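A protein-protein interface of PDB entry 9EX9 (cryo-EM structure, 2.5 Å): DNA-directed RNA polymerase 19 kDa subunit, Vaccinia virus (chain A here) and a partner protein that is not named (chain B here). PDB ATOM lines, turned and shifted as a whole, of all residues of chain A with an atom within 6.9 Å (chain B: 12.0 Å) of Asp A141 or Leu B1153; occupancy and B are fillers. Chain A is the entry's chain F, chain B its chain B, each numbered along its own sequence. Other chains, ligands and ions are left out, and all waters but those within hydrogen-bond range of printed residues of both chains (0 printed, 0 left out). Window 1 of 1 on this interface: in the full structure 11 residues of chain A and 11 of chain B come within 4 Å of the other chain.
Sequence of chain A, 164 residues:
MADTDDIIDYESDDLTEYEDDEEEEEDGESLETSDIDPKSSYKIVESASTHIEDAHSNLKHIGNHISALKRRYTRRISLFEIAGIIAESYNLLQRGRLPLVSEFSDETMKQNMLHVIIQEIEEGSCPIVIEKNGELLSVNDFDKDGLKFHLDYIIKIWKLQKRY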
ATOM      1  N   THR A  74      19.424 -12.207  10.916  1.00  0.00           N
ATOM      2  CA  THR A  74      20.731 -11.606  11.167  1.00  0.00           C
ATOM      3  C   THR A  74      20.891 -11.090  12.595  1.00  0.00           C
ATOM      4  O   THR A  74      22.024 -10.886  13.039  1.00  0.00           O
ATOM      5  CB  THR A  74      20.967 -10.455  10.187  1.00  0.00           C
ATOM      6  OG1 THR A  74      21.064 -10.971   8.858  1.00  0.00           O
ATOM      7  CG2 THR A  74      22.239  -9.697  10.526  1.00  0.00           C
ATOM      8  N   ARG A  75      19.800 -10.872  13.324  1.00  0.00           N
ATOM      9  CA  ARG A  75      19.856 -10.143  14.584  1.00  0.00           C
ATOM     10  C   ARG A  75      20.137 -11.021  15.795  1.00  0.00           C
ATOM     11  O   ARG A  75      20.175 -10.499  16.912  1.00  0.00           O
ATOM     12  CB  ARG A  75      18.546  -9.392  14.814  1.00  0.00           C
ATOM     13  CG  ARG A  75      18.200  -8.405  13.729  1.00  0.00           C
ATOM     14  CD  ARG A  75      19.247  -7.322  13.578  1.00  0.00           C
ATOM     15  NE  ARG A  75      18.861  -6.359  12.554  1.00  0.00           N
ATOM     16  CZ  ARG A  75      18.202  -5.231  12.784  1.00  0.00           C
ATOM     17  NH1 ARG A  75      17.877  -4.852  14.008  1.00  0.00           N
ATOM     18  NH2 ARG A  75      17.858  -4.461  11.757  1.00  0.00           N
ATOM     19  N   ARG A  76      20.324 -12.323  15.624  1.00  0.00           N
ATOM     20  CA  ARG A  76      20.613 -13.179  16.765  1.00  0.00           C
ATOM     21  C   ARG A  76      22.095 -13.122  17.108  1.00  0.00           C
ATOM     22  O   ARG A  76      22.944 -12.899  16.245  1.00  0.00           O
ATOM     23  CB  ARG A  76      20.167 -14.620  16.504  1.00  0.00           C
ATOM     24  CG  ARG A  76      20.553 -15.201  15.160  1.00  0.00           C
ATOM     25  CD  ARG A  76      19.706 -16.405  14.815  1.00  0.00           C
ATOM     26  NE  ARG A  76      20.070 -17.560  15.621  1.00  0.00           N
ATOM     27  CZ  ARG A  76      21.180 -18.263  15.452  1.00  0.00           C
ATOM     28  NH1 ARG A  76      22.061 -17.949  14.520  1.00  0.00           N
ATOM     29  NH2 ARG A  76      21.411 -19.309  16.238  1.00  0.00           N
ATOM     30  N   GLU A 135      25.768  -5.983   6.561  1.00  0.00           N
ATOM     31  CA  GLU A 135      25.234  -4.868   7.323  1.00  0.00           C
ATOM     32  C   GLU A 135      26.223  -4.488   8.413  1.00  0.00           C
ATOM     33  O   GLU A 135      27.198  -5.193   8.671  1.00  0.00           O
ATOM     34  CB  GLU A 135      23.876  -5.221   7.936  1.00  0.00           C
ATOM     35  CG  GLU A 135      22.861  -5.683   6.916  1.00  0.00           C
ATOM     36  CD  GLU A 135      21.495  -5.913   7.515  1.00  0.00           C
ATOM     37  OE1 GLU A 135      21.181  -5.288   8.546  1.00  0.00           O
ATOM     38  OE2 GLU A 135      20.733  -6.723   6.953  1.00  0.00           O
ATOM     39  N   LEU A 136      25.968  -3.348   9.047  1.00  0.00           N
ATOM     40  CA  LEU A 136      26.816  -2.822  10.110  1.00  0.00           C
ATOM     41  C   LEU A 136      25.961  -2.616  11.349  1.00  0.00           C
ATOM     42  O   LEU A 136      25.014  -1.824  11.328  1.00  0.00           O
ATOM     43  CB  LEU A 136      27.475  -1.514   9.672  1.00  0.00           C
ATOM     44  CG  LEU A 136      28.414  -1.670   8.475  1.00  0.00           C
ATOM     45  CD1 LEU A 136      28.609  -0.357   7.754  1.00  0.00           C
ATOM     46  CD2 LEU A 136      29.743  -2.217   8.937  1.00  0.00           C
ATOM     47  N   LEU A 137      26.297  -3.323  12.423  1.00  0.00           N
ATOM     48  CA  LEU A 137      25.492  -3.354  13.635  1.00  0.00           C
ATOM     49  C   LEU A 137      26.297  -2.865  14.828  1.00  0.00           C
ATOM     50  O   LEU A 137      27.458  -3.241  15.003  1.00  0.00           O
ATOM     51  CB  LEU A 137      24.984  -4.768  13.929  1.00  0.00           C
ATOM     52  CG  LEU A 137      23.868  -5.329  13.054  1.00  0.00           C
ATOM     53  CD1 LEU A 137      24.382  -5.741  11.700  1.00  0.00           C
ATOM     54  CD2 LEU A 137      23.231  -6.502  13.747  1.00  0.00           C
ATOM     55  N   SER A 138      25.674  -2.032  15.649  1.00  0.00           N
ATOM     56  CA  SER A 138      26.199  -1.733  16.968  1.00  0.00           C
ATOM     57  C   SER A 138      25.696  -2.780  17.955  1.00  0.00           C
ATOM     58  O   SER A 138      24.754  -3.522  17.683  1.00  0.00           O
ATOM     59  CB  SER A 138      25.787  -0.331  17.406  1.00  0.00           C
ATOM     60  OG  SER A 138      24.379  -0.201  17.436  1.00  0.00           O
ATOM     61  N   VAL A 139      26.333  -2.833  19.126  1.00  0.00           N
ATOM     62  CA  VAL A 139      26.014  -3.885  20.081  1.00  0.00           C
ATOM     63  C   VAL A 139      24.566  -3.815  20.541  1.00  0.00           C
ATOM     64  O   VAL A 139      24.072  -4.760  21.161  1.00  0.00           O
ATOM     65  CB  VAL A 139      26.969  -3.823  21.288  1.00  0.00           C
ATOM     66  CG1 VAL A 139      26.624  -2.648  22.180  1.00  0.00           C
ATOM     67  CG2 VAL A 139      26.914  -5.118  22.065  1.00  0.00           C
ATOM     68  N   ASN A 140      23.870  -2.718  20.259  1.00  0.00           N
ATOM     69  CA  ASN A 140      22.484  -2.570  20.674  1.00  0.00           C
ATOM     70  C   ASN A 140      21.485  -2.943  19.590  1.00  0.00           C
ATOM     71  O   ASN A 140      20.279  -2.895  19.848  1.00  0.00           O
ATOM     72  CB  ASN A 140      22.223  -1.133  21.120  1.00  0.00           C
ATOM     73  CG  ASN A 140      23.113  -0.712  22.264  1.00  0.00           C
ATOM     74  OD1 ASN A 140      23.992   0.131  22.101  1.00  0.00           O
ATOM     75  ND2 ASN A 140      22.891  -1.299  23.432  1.00  0.00           N
ATOM     76  N   ASP A 141      21.940  -3.307  18.392  1.00  0.00           N
ATOM     77  CA  ASP A 141      21.024  -3.736  17.342  1.00  0.00           C
ATOM     78  C   ASP A 141      20.729  -5.227  17.378  1.00  0.00           C
ATOM     79  O   ASP A 141      19.827  -5.676  16.668  1.00  0.00           O
ATOM     80  CB  ASP A 141      21.581  -3.366  15.969  1.00  0.00           C
ATOM     81  CG  ASP A 141      21.521  -1.882  15.702  1.00  0.00           C
ATOM     82  OD1 ASP A 141      20.685  -1.203  16.328  1.00  0.00           O
ATOM     83  OD2 ASP A 141      22.305  -1.390  14.867  1.00  0.00           O
ATOM     84  N   PHE A 142      21.458  -6.002  18.175  1.00  0.00           N
ATOM     85  CA  PHE A 142      21.134  -7.406  18.353  1.00  0.00           C
ATOM     86  C   PHE A 142      19.927  -7.555  19.273  1.00  0.00           C
ATOM     87  O   PHE A 142      19.520  -6.623  19.968  1.00  0.00           O
ATOM     88  CB  PHE A 142      22.322  -8.165  18.934  1.00  0.00           C
ATOM     89  CG  PHE A 142      23.513  -8.205  18.032  1.00  0.00           C
ATOM     90  CD1 PHE A 142      23.524  -9.014  16.916  1.00  0.00           C
ATOM     91  CD2 PHE A 142      24.627  -7.438  18.304  1.00  0.00           C
ATOM     92  CE1 PHE A 142      24.617  -9.055  16.089  1.00  0.00           C
ATOM     93  CE2 PHE A 142      25.723  -7.475  17.478  1.00  0.00           C
ATOM     94  CZ  PHE A 142      25.717  -8.284  16.370  1.00  0.00           C
ATOM     95  N   ASP A 143      19.350  -8.753  19.273  1.00  0.00           N
ATOM     96  CA  ASP A 143      18.234  -9.031  20.164  1.00  0.00           C
ATOM     97  C   ASP A 143      18.652  -8.789  21.608  1.00  0.00           C
ATOM     98  O   ASP A 143      19.737  -9.188  22.034  1.00  0.00           O
ATOM     99  CB  ASP A 143      17.755 -10.468  19.978  1.00  0.00           C
ATOM    100  CG  ASP A 143      16.572 -10.803  20.853  1.00  0.00           C
ATOM    101  OD1 ASP A 143      15.691  -9.938  21.015  1.00  0.00           O
ATOM    102  OD2 ASP A 143      16.515 -11.934  21.372  1.00  0.00           O
ATOM    103  N   LYS A 144      17.782  -8.121  22.363  1.00  0.00           N
ATOM    104  CA  LYS A 144      18.149  -7.693  23.708  1.00  0.00           C
ATOM    105  C   LYS A 144      18.259  -8.875  24.666  1.00  0.00           C
ATOM    106  O   LYS A 144      19.176  -8.927  25.499  1.00  0.00           O
ATOM    107  CB  LYS A 144      17.129  -6.678  24.215  1.00  0.00           C
ATOM    108  CG  LYS A 144      17.538  -5.976  25.491  1.00  0.00           C
ATOM    109  CD  LYS A 144      16.464  -5.007  25.949  1.00  0.00           C
ATOM    110  CE  LYS A 144      16.833  -4.353  27.270  1.00  0.00           C
ATOM    111  NZ  LYS A 144      15.777  -3.415  27.736  1.00  0.00           N
ATOM    112  N   PHE B1149      29.649   3.877   6.077  1.00  0.00           N
ATOM    113  CA  PHE B1149      28.970   4.733   7.040  1.00  0.00           C
ATOM    114  C   PHE B1149      27.916   3.939   7.792  1.00  0.00           C
ATOM    115  O   PHE B1149      27.253   3.071   7.218  1.00  0.00           O
ATOM    116  CB  PHE B1149      28.313   5.923   6.346  1.00  0.00           C
ATOM    117  CG  PHE B1149      29.267   6.755   5.554  1.00  0.00           C
ATOM    118  CD1 PHE B1149      29.576   6.423   4.251  1.00  0.00           C
ATOM    119  CD2 PHE B1149      29.862   7.867   6.115  1.00  0.00           C
ATOM    120  CE1 PHE B1149      30.456   7.184   3.522  1.00  0.00           C
ATOM    121  CE2 PHE B1149      30.744   8.630   5.390  1.00  0.00           C
ATOM    122  CZ  PHE B1149      31.040   8.290   4.092  1.00  0.00           C
ATOM    123  N   TYR B1150      27.758   4.249   9.075  1.00  0.00           N
ATOM    124  CA  TYR B1150      26.763   3.580   9.899  1.00  0.00           C
ATOM    125  C   TYR B1150      25.399   4.228   9.725  1.00  0.00           C
ATOM    126  O   TYR B1150      25.281   5.453   9.653  1.00  0.00           O
ATOM    127  CB  TYR B1150      27.168   3.623  11.370  1.00  0.00           C
ATOM    128  CG  TYR B1150      26.119   3.053  12.291  1.00  0.00           C
ATOM    129  CD1 TYR B1150      25.998   1.685  12.472  1.00  0.00           C
ATOM    130  CD2 TYR B1150      25.249   3.881  12.980  1.00  0.00           C
ATOM    131  CE1 TYR B1150      25.041   1.159  13.310  1.00  0.00           C
ATOM    132  CE2 TYR B1150      24.289   3.363  13.822  1.00  0.00           C
ATOM    133  CZ  TYR B1150      24.189   2.003  13.983  1.00  0.00           C
ATOM    134  OH  TYR B1150      23.233   1.485  14.821  1.00  0.00           O
ATOM    135  N   LYS B1151      24.365   3.394   9.665  1.00  0.00           N
ATOM    136  CA  LYS B1151      22.996   3.851   9.515  1.00  0.00           C
ATOM    137  C   LYS B1151      22.146   3.275  10.638  1.00  0.00           C
ATOM    138  O   LYS B1151      22.345   2.122  11.032  1.00  0.00           O
ATOM    139  CB  LYS B1151      22.417   3.419   8.163  1.00  0.00           C
ATOM    140  CG  LYS B1151      23.307   3.735   6.978  1.00  0.00           C
ATOM    141  CD  LYS B1151      22.745   3.145   5.697  1.00  0.00           C
ATOM    142  CE  LYS B1151      23.689   3.364   4.525  1.00  0.00           C
ATOM    143  NZ  LYS B1151      23.169   2.759   3.268  1.00  0.00           N
ATOM    144  N   PRO B1152      21.200   4.041  11.178  1.00  0.00           N
ATOM    145  CA  PRO B1152      20.311   3.482  12.200  1.00  0.00           C
ATOM    146  C   PRO B1152      19.505   2.314  11.653  1.00  0.00           C
ATOM    147  O   PRO B1152      19.129   2.289  10.480  1.00  0.00           O
ATOM    148  CB  PRO B1152      19.411   4.663  12.573  1.00  0.00           C
ATOM    149  CG  PRO B1152      20.201   5.863  12.218  1.00  0.00           C
ATOM    150  CD  PRO B1152      20.985   5.487  11.003  1.00  0.00           C
ATOM    151  N   LEU B1153      19.241   1.343  12.522  1.00  0.00           N
ATOM    152  CA  LEU B1153      18.493   0.147  12.171  1.00  0.00           C
ATOM    153  C   LEU B1153      17.281   0.018  13.083  1.00  0.00           C
ATOM    154  O   LEU B1153      17.370   0.269  14.287  1.00  0.00           O
ATOM    155  CB  LEU B1153      19.369  -1.103  12.290  1.00  0.00           C
ATOM    156  CG  LEU B1153      20.568  -1.187  11.345  1.00  0.00           C
ATOM    157  CD1 LEU B1153      21.432  -2.386  11.680  1.00  0.00           C
ATOM    158  CD2 LEU B1153      20.109  -1.256   9.903  1.00  0.00           C
ATOM    159  N   ASP B1154      16.151  -0.373  12.501  1.00  0.00           N
ATOM    160  CA  ASP B1154      14.936  -0.558  13.277  1.00  0.00           C
ATOM    161  C   ASP B1154      15.069  -1.772  14.192  1.00  0.00           C
ATOM    162  O   ASP B1154      15.918  -2.643  13.994  1.00  0.00           O
ATOM    163  CB  ASP B1154      13.729  -0.721  12.355  1.00  0.00           C
ATOM    164  CG  ASP B1154      13.956  -1.755  11.278  1.00  0.00           C
ATOM    165  OD1 ASP B1154      15.126  -1.965  10.898  1.00  0.00           O
ATOM    166  OD2 ASP B1154      12.968  -2.354  10.808  1.00  0.00           O
ATOM    167  N   LYS B1155      14.213  -1.819  15.209  1.00  0.00           N
ATOM    168  CA  LYS B1155      14.321  -2.839  16.240  1.00  0.00           C
ATOM    169  C   LYS B1155      13.697  -4.154  15.791  1.00  0.00           C
ATOM    170  O   LYS B1155      12.772  -4.186  14.975  1.00  0.00           O
ATOM    171  CB  LYS B1155      13.653  -2.368  17.532  1.00  0.00           C
ATOM    172  CG  LYS B1155      14.280  -1.122  18.142  1.00  0.00           C
ATOM    173  CD  LYS B1155      15.724  -1.358  18.563  1.00  0.00           C
ATOM    174  CE  LYS B1155      16.347  -0.102  19.152  1.00  0.00           C
ATOM    175  NZ  LYS B1155      17.806  -0.268  19.405  1.00  0.00           N
ATOM    176  N   VAL B1156      14.223  -5.248  16.338  1.00  0.00           N
ATOM    177  CA  VAL B1156      13.728  -6.595  16.085  1.00  0.00           C
ATOM    178  C   VAL B1156      13.603  -7.315  17.419  1.00  0.00           C
ATOM    179  O   VAL B1156      14.483  -7.203  18.278  1.00  0.00           O
ATOM    180  CB  VAL B1156      14.658  -7.370  15.130  1.00  0.00           C
ATOM    181  CG1 VAL B1156      14.125  -8.762  14.886  1.00  0.00           C
ATOM    182  CG2 VAL B1156      14.804  -6.625  13.822  1.00  0.00           C
ATOM    183  N   ASP B1157      12.510  -8.061  17.591  1.00  0.00           N
ATOM    184  CA  ASP B1157      12.202  -8.692  18.872  1.00  0.00           C
ATOM    185  C   ASP B1157      12.747 -10.116  18.962  1.00  0.00           C
ATOM    186  O   ASP B1157      13.546 -10.423  19.849  1.00  0.00           O
ATOM    187  CB  ASP B1157      10.689  -8.689  19.103  1.00  0.00           C
ATOM    188  CG  ASP B1157      10.305  -9.319  20.422  1.00  0.00           C
ATOM    189  OD1 ASP B1157      10.865  -8.910  21.459  1.00  0.00           O
ATOM    190  OD2 ASP B1157       9.440 -10.219  20.425  1.00  0.00           O
ATOM    191  N   LEU B1158      12.312 -10.995  18.062  1.00  0.00           N
ATOM    192  CA  LEU B1158      12.782 -12.374  17.911  1.00  0.00           C
ATOM    193  C   LEU B1158      12.172 -13.341  18.925  1.00  0.00           C
ATOM    194  O   LEU B1158      12.489 -14.528  18.866  1.00  0.00           O
ATOM    195  CB  LEU B1158      14.314 -12.481  18.001  1.00  0.00           C
ATOM    196  CG  LEU B1158      15.054 -13.070  16.799  1.00  0.00           C
ATOM    197  CD1 LEU B1158      14.729 -12.326  15.525  1.00  0.00           C
ATOM    198  CD2 LEU B1158      16.542 -13.035  17.051  1.00  0.00           C
ATOM    199  N   LYS B1159      11.318 -12.893  19.837  1.00  0.00           N
ATOM    200  CA  LYS B1159      10.674 -13.796  20.780  1.00  0.00           C
ATOM    201  C   LYS B1159       9.382 -14.354  20.199  1.00  0.00           C
ATOM    202  O   LYS B1159       8.792 -13.766  19.289  1.00  0.00           O
ATOM    203  CB  LYS B1159      10.383 -13.069  22.087  1.00  0.00           C
ATOM    204  CG  LYS B1159      11.625 -12.583  22.805  1.00  0.00           C
ATOM    205  CD  LYS B1159      11.282 -11.621  23.929  1.00  0.00           C
ATOM    206  CE  LYS B1159      10.569 -12.319  25.071  1.00  0.00           C
ATOM    207  NZ  LYS B1159      11.394 -13.408  25.660  1.00  0.00           N
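OD1 of Asp B1154 lies within salt-bridge range of NH2 of Arg A75 (3.8 Å).
The side-chain hydroxyl (OH) of Tyr B1150 lies within hydrogen-bond range of the side-chain hydroxyl (OG) of Ser A138.
OD2 of Asp A141 lies within hydrogen-bond range of OH of Tyr B1150, 3.0 Å away.
O of Asp B1157 lies close to OD1 of Asp A143.
Asp A141 touches two residues of chain B.
Leu B1153 touches just these residues of chain A: Arg A75 (3.7 Å), Leu A136 (3.6 Å) and Asp A141 (3.5 Å).
Of the printed residues of chain B, Arg A75 touches Leu B1153, Asp B1154 and Val B1156.
Glu A135 touches none of the printed residues of chain B.
Leu A137 touches none of the printed residues of chain B.
Of chain B, only Tyr B1150 (3.3 Å) comes within 4 Å of Ser A138.
No residue of chain B comes within 4 Å of Val A139.
No residue of chain B comes within 4 Å of Phe A142.
Of the printed residues of chain A, Val B1156 touches Arg A75.
Of the printed residues of chain A, Asp B1157 touches Asp A143 (2.5 Å).
Leu B1153 touches Arg A75 (CB to NH2, 3.7 Å).
Arg A75 touches Val B1156.
Arg A76 touches Leu B1158 (CB to CD2, 3.99 Å).
Leu A136 touches Phe B1149.
CE1 of Tyr B1150 touches O of Leu A136, at 3.6 Å.
O of Leu A136 touches CD1 of Leu B1153 (3.6 Å).
O of Asn A140 touches NZ of Lys B1155, 3.6 Å away.
Asp A141 touches Leu B1153.
O of Arg A75 sits at hydrogen-bond distance from N of Asp A143 (3.1 Å).
The guanidinium group (NH1) of Arg A75 lies within hydrogen-bond range of the backbone carbonyl oxygen (O) of Asp A141, 3.4 Å away.
N of Lys B1159 lies close to OD2 of Asp B1157 (3.3 Å).
Of the 11 printed residues of chain B, 8 touch a printed residue of chain A.
Of the 13 printed residues of chain A, 7 touch a printed residue of chain B.
Among the printed residues, Asp or Glu carboxylates within 4 Å of a Lys or Arg side-chain nitrogen of the other chain: Arg A75 with Asp B1154 (3.8 Å).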
